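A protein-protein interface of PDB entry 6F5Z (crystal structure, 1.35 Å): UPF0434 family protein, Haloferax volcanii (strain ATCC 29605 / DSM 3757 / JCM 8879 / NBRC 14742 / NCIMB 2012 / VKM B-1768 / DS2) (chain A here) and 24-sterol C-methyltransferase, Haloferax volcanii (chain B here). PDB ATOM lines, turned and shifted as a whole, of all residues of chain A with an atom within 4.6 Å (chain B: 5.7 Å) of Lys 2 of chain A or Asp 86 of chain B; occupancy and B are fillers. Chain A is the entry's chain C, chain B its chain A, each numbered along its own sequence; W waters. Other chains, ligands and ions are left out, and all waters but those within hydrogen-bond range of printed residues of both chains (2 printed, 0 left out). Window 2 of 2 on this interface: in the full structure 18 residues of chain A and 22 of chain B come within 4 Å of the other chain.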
ATOM      1  N   MET A   1     -22.695  18.521 -14.533  1.00  0.00           N
ATOM      2  CA  MET A   1     -23.042  18.809 -15.933  1.00  0.00           C
ATOM      3  C   MET A   1     -23.515  20.256 -16.011  1.00  0.00           C
ATOM      4  O   MET A   1     -24.274  20.698 -15.153  1.00  0.00           O
ATOM      5  CB  MET A   1     -24.162  17.868 -16.424  1.00  0.00           C
ATOM      6  CG  MET A   1     -24.651  18.196 -17.842  1.00  0.00           C
ATOM      7  SD  MET A   1     -25.981  17.114 -18.446  1.00  0.00           S
ATOM      8  CE  MET A   1     -25.044  15.546 -18.820  1.00  0.00           C
ATOM      9  N   LYS A   2     -23.146  20.963 -17.089  1.00  0.00           N
ATOM     10  CA  LYS A   2     -23.606  22.340 -17.274  1.00  0.00           C
ATOM     11  C   LYS A   2     -25.111  22.397 -17.421  1.00  0.00           C
ATOM     12  O   LYS A   2     -25.680  21.643 -18.209  1.00  0.00           O
ATOM     13  CB  LYS A   2     -22.977  22.914 -18.556  1.00  0.00           C
ATOM     14  CG  LYS A   2     -21.554  23.366 -18.413  1.00  0.00           C
ATOM     15  CD  LYS A   2     -21.058  23.803 -19.827  1.00  0.00           C
ATOM     16  CE  LYS A   2     -20.049  24.913 -19.810  1.00  0.00           C
ATOM     17  NZ  LYS A   2     -20.698  26.256 -19.743  1.00  0.00           N
ATOM     18  N   GLU A   3     -25.769  23.333 -16.731  1.00  0.00           N
ATOM     19  CA  GLU A   3     -27.216  23.500 -16.863  1.00  0.00           C
ATOM     20  C   GLU A   3     -27.598  23.845 -18.314  1.00  0.00           C
ATOM     21  O   GLU A   3     -28.634  23.392 -18.810  1.00  0.00           O
ATOM     22  CB  GLU A   3     -27.707  24.563 -15.860  1.00  0.00           C
ATOM     23  CG  GLU A   3     -29.198  24.788 -15.928  1.00  0.00           C
ATOM     24  CD  GLU A   3     -29.713  25.819 -14.942  1.00  0.00           C
ATOM     25  OE1 GLU A   3     -28.912  26.338 -14.132  1.00  0.00           O
ATOM     26  OE2 GLU A   3     -30.940  26.052 -14.927  1.00  0.00           O
ATOM     27  N   SER A   4     -26.739  24.610 -19.008  1.00  0.00           N
ATOM     28  CA  SER A   4     -26.961  24.937 -20.428  1.00  0.00           C
ATOM     29  C   SER A   4     -26.984  23.694 -21.353  1.00  0.00           C
ATOM     30  O   SER A   4     -27.527  23.784 -22.453  1.00  0.00           O
ATOM     31  CB  SER A   4     -25.920  25.942 -20.934  1.00  0.00           C
ATOM     32  OG  SER A   4     -24.642  25.345 -20.857  1.00  0.00           O
ATOM     33  N   LEU A   5     -26.377  22.559 -20.950  1.00  0.00           N
ATOM     34  CA  LEU A   5     -26.392  21.330 -21.758  1.00  0.00           C
ATOM     35  C   LEU A   5     -27.651  20.522 -21.497  1.00  0.00           C
ATOM     36  O   LEU A   5     -27.974  19.617 -22.259  1.00  0.00           O
ATOM     37  CB  LEU A   5     -25.169  20.446 -21.439  1.00  0.00           C
ATOM     38  CG  LEU A   5     -23.875  20.697 -22.247  1.00  0.00           C
ATOM     39  CD1 LEU A   5     -23.482  22.162 -22.283  1.00  0.00           C
ATOM     40  CD2 LEU A   5     -22.741  19.904 -21.660  1.00  0.00           C
ATOM     41  N   MET A   6     -28.395  20.841 -20.424  1.00  0.00           N
ATOM     42  CA  MET A   6     -29.583  20.056 -20.077  1.00  0.00           C
ATOM     43  C   MET A   6     -30.811  20.373 -20.879  1.00  0.00           C
ATOM     44  O   MET A   6     -31.806  19.663 -20.760  1.00  0.00           O
ATOM     45  CB  MET A   6     -29.881  20.229 -18.587  1.00  0.00           C
ATOM     46  CG  MET A   6     -28.739  19.781 -17.740  1.00  0.00           C
ATOM     47  SD  MET A   6     -29.152  20.021 -15.993  1.00  0.00           S
ATOM     48  CE  MET A   6     -27.698  19.431 -15.259  1.00  0.00           C
ATOM     49  N   ASP A  28     -22.441  27.618 -14.120  1.00  0.00           N
ATOM     50  CA  ASP A  28     -23.299  26.792 -14.972  1.00  0.00           C
ATOM     51  C   ASP A  28     -23.254  25.334 -14.561  1.00  0.00           C
ATOM     52  O   ASP A  28     -24.172  24.583 -14.871  1.00  0.00           O
ATOM     53  CB  ASP A  28     -22.838  26.911 -16.438  1.00  0.00           C
ATOM     54  CG  ASP A  28     -23.790  26.461 -17.542  1.00  0.00           C
ATOM     55  OD1 ASP A  28     -25.008  26.320 -17.270  1.00  0.00           O
ATOM     56  OD2 ASP A  28     -23.338  26.385 -18.705  1.00  0.00           O
ATOM     57  N   GLU A  29     -22.185  24.926 -13.878  1.00  0.00           N
ATOM     58  CA  GLU A  29     -22.020  23.526 -13.491  1.00  0.00           C
ATOM     59  C   GLU A  29     -22.982  23.079 -12.379  1.00  0.00           C
ATOM     60  O   GLU A  29     -22.912  23.598 -11.279  1.00  0.00           O
ATOM     61  CB  GLU A  29     -20.551  23.271 -13.072  1.00  0.00           C
ATOM     62  CG  GLU A  29     -20.249  21.811 -12.754  1.00  0.00           C
ATOM     63  CD  GLU A  29     -20.376  20.838 -13.911  1.00  0.00           C
ATOM     64  OE1 GLU A  29     -20.445  21.283 -15.080  1.00  0.00           O
ATOM     65  OE2 GLU A  29     -20.357  19.616 -13.643  1.00  0.00           O
ATOM     66  N   ILE B  62     -15.864  20.685 -31.383  1.00  0.00           N
ATOM     67  CA  ILE B  62     -17.273  20.547 -31.000  1.00  0.00           C
ATOM     68  C   ILE B  62     -17.659  21.484 -29.848  1.00  0.00           C
ATOM     69  O   ILE B  62     -16.827  21.739 -28.962  1.00  0.00           O
ATOM     70  CB  ILE B  62     -17.678  19.088 -30.694  1.00  0.00           C
ATOM     71  CG1 ILE B  62     -16.867  18.476 -29.534  1.00  0.00           C
ATOM     72  CG2 ILE B  62     -17.559  18.244 -31.951  1.00  0.00           C
ATOM     73  CD1 ILE B  62     -17.538  17.193 -28.873  1.00  0.00           C
ATOM     74  N   GLY B  63     -18.902  21.964 -29.888  1.00  0.00           N
ATOM     75  CA  GLY B  63     -19.421  22.877 -28.875  1.00  0.00           C
ATOM     76  C   GLY B  63     -19.886  22.178 -27.626  1.00  0.00           C
ATOM     77  O   GLY B  63     -19.637  22.668 -26.522  1.00  0.00           O
ATOM     78  N   ARG B  64     -20.557  21.021 -27.784  1.00  0.00           N
ATOM     79  CA  ARG B  64     -21.157  20.287 -26.682  1.00  0.00           C
ATOM     80  C   ARG B  64     -20.976  18.826 -26.951  1.00  0.00           C
ATOM     81  O   ARG B  64     -21.228  18.382 -28.059  1.00  0.00           O
ATOM     82  CB  ARG B  64     -22.665  20.589 -26.638  1.00  0.00           C
ATOM     83  CG  ARG B  64     -22.986  22.087 -26.570  1.00  0.00           C
ATOM     84  CD  ARG B  64     -24.353  22.349 -26.003  1.00  0.00           C
ATOM     85  NE  ARG B  64     -25.432  21.737 -26.783  1.00  0.00           N
ATOM     86  CZ  ARG B  64     -26.704  21.806 -26.423  1.00  0.00           C
ATOM     87  NH1 ARG B  64     -27.054  22.465 -25.328  1.00  0.00           N
ATOM     88  NH2 ARG B  64     -27.637  21.231 -27.161  1.00  0.00           N
ATOM     89  N   GLY B  65     -20.592  18.079 -25.936  1.00  0.00           N
ATOM     90  CA  GLY B  65     -20.441  16.638 -26.088  1.00  0.00           C
ATOM     91  C   GLY B  65     -21.089  15.939 -24.919  1.00  0.00           C
ATOM     92  O   GLY B  65     -21.039  16.462 -23.795  1.00  0.00           O
ATOM     93  N   THR B  84     -12.396  19.518 -19.267  1.00  0.00           N
ATOM     94  CA  THR B  84     -13.260  20.601 -19.774  1.00  0.00           C
ATOM     95  C   THR B  84     -14.711  20.286 -19.479  1.00  0.00           C
ATOM     96  O   THR B  84     -15.115  19.119 -19.606  1.00  0.00           O
ATOM     97  CB  THR B  84     -13.078  20.820 -21.277  1.00  0.00           C
ATOM     98  OG1 THR B  84     -14.100  21.729 -21.730  1.00  0.00           O
ATOM     99  CG2 THR B  84     -13.189  19.511 -22.080  1.00  0.00           C
ATOM    100  N   ASP B  85     -15.522  21.323 -19.181  1.00  0.00           N
ATOM    101  CA  ASP B  85     -16.945  21.136 -18.896  1.00  0.00           C
ATOM    102  C   ASP B  85     -17.820  21.214 -20.149  1.00  0.00           C
ATOM    103  O   ASP B  85     -19.028  20.985 -20.064  1.00  0.00           O
ATOM    104  CB  ASP B  85     -17.423  22.091 -17.792  1.00  0.00           C
ATOM    105  CG  ASP B  85     -16.762  21.794 -16.449  1.00  0.00           C
ATOM    106  OD1 ASP B  85     -16.812  20.622 -16.005  1.00  0.00           O
ATOM    107  OD2 ASP B  85     -16.180  22.726 -15.854  1.00  0.00           O
ATOM    108  N   ASP B  86     -17.200  21.451 -21.332  1.00  0.00           N
ATOM    109  CA  ASP B  86     -17.931  21.453 -22.605  1.00  0.00           C
ATOM    110  C   ASP B  86     -18.319  20.014 -22.955  1.00  0.00           C
ATOM    111  O   ASP B  86     -19.204  19.788 -23.781  1.00  0.00           O
ATOM    112  CB  ASP B  86     -17.075  22.089 -23.722  1.00  0.00           C
ATOM    113  CG  ASP B  86     -16.794  23.580 -23.518  1.00  0.00           C
ATOM    114  OD1 ASP B  86     -17.578  24.247 -22.797  1.00  0.00           O
ATOM    115  OD2 ASP B  86     -15.810  24.085 -24.101  1.00  0.00           O
ATOM    116  N   LEU B  87     -17.644  19.041 -22.312  1.00  0.00           N
ATOM    117  CA  LEU B  87     -17.928  17.617 -22.465  1.00  0.00           C
ATOM    118  C   LEU B  87     -18.561  17.156 -21.172  1.00  0.00           C
ATOM    119  O   LEU B  87     -18.018  17.393 -20.079  1.00  0.00           O
ATOM    120  CB  LEU B  87     -16.646  16.831 -22.719  1.00  0.00           C
ATOM    121  CG  LEU B  87     -15.855  17.286 -23.964  1.00  0.00           C
ATOM    122  CD1 LEU B  87     -14.623  16.414 -24.156  1.00  0.00           C
ATOM    123  CD2 LEU B  87     -16.705  17.240 -25.242  1.00  0.00           C
ATOM    124  N   SER B  88     -19.738  16.603 -21.275  1.00  0.00           N
ATOM    125  CA  SER B  88     -20.483  16.122 -20.119  1.00  0.00           C
ATOM    126  C   SER B  88     -20.662  14.624 -20.236  1.00  0.00           C
ATOM    127  O   SER B  88     -20.549  14.063 -21.324  1.00  0.00           O
ATOM    128  CB  SER B  88     -21.849  16.773 -20.044  1.00  0.00           C
ATOM    129  OG  SER B  88     -22.667  16.312 -21.108  1.00  0.00           O
HETATM  130  O   HOH W   1     -20.917  19.775 -18.457  1.00  0.00           O
HETATM  131  O   HOH W   2     -19.172  19.345 -16.377  1.00  0.00           O
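Met 1 of chain A touches Ser 88 of chain B. Lys 2 of chain A touches Asp 85 of chain B. Lys 2 of chain A touches Asp 86 of chain B. Leu 5 of chain A touches Arg 64 of chain B (CA to NH1, 3.8 Å). Leu 5 of chain A touches Ser 88 of chain B (CD2 to CB, 3.6 Å). Asp 85 of chain B touches Glu 29 of chain A.
The backbone carbonyl oxygen (O) of Asp 86 of chain B sits at hydrogen-bond distance from the backbone NH (N) of Gly 65 of chain B, at 3.1 Å. The backbone carbonyl oxygen (O) of Gly 65 of chain B lies within hydrogen-bond range of the backbone NH (N) of Ser 88 of chain B (2.8 Å). N of Asp 86 of chain B is in hydrogen-bond range of OG1 of Thr 84 of chain B (3.1 Å). The side-chain carboxylate (OE2) of Glu 29 of chain A sits at hydrogen-bond distance from the backbone NH (N) of Met 1 of chain A, 2.7 Å away. The side-chain carboxylate of Asp 28 of chain A is in salt-bridge range of the side-chain amino group of Lys 2 of chain A (2.8 Å). The side-chain carboxylate (OD2) of Asp 28 of chain A is in hydrogen-bond range of the side-chain hydroxyl (OG) of Ser 4 of chain A (2.7 Å).
Water W2 bridges the side-chain carboxylate of Glu 29 of chain A (2.7 Å) and the side-chain carboxylate of Asp 85 of chain B (2.7 Å). Water W1 lies within hydrogen-bond range of the backbone carbonyl oxygen of Asp 85 of chain B (2.8 Å) and the backbone NH of Lys 2 of chain A (2.9 Å).
Of the 9 printed residues of chain B, 4 touch a printed residue of chain A. Hydrophobic or aromatic side chains of chain A within 4 Å of the printed part of chain B: Met 1 and Leu 5. Among the printed residues, 7 pairs touch across the chains.
Lys 2 of chain A touches just these residues of chain B: Asp 85 (3.5 Å) and Asp 86 (3.9 Å). Of the printed residues of chain B, Ser 4 of chain A touches Arg 64. Printed residues of chain A within 4 Å of Ser 88 of chain B: Met 1 and Leu 5. Printed residues of chain B within 4 Å of Glu 29 of chain A: Asp 85. Printed residues of chain A within 4 Å of Asp 85 of chain B: Lys 2 and Glu 29. Of the printed residues of chain B, Leu 5 of chain A touches Arg 64 and Ser 88. Gly 65 of chain B touches none of the printed residues of chain A.
NH1 of Arg 64 of chain B is in hydrogen-bond range of O of Ser 4 of chain A, 3.2 Å away.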
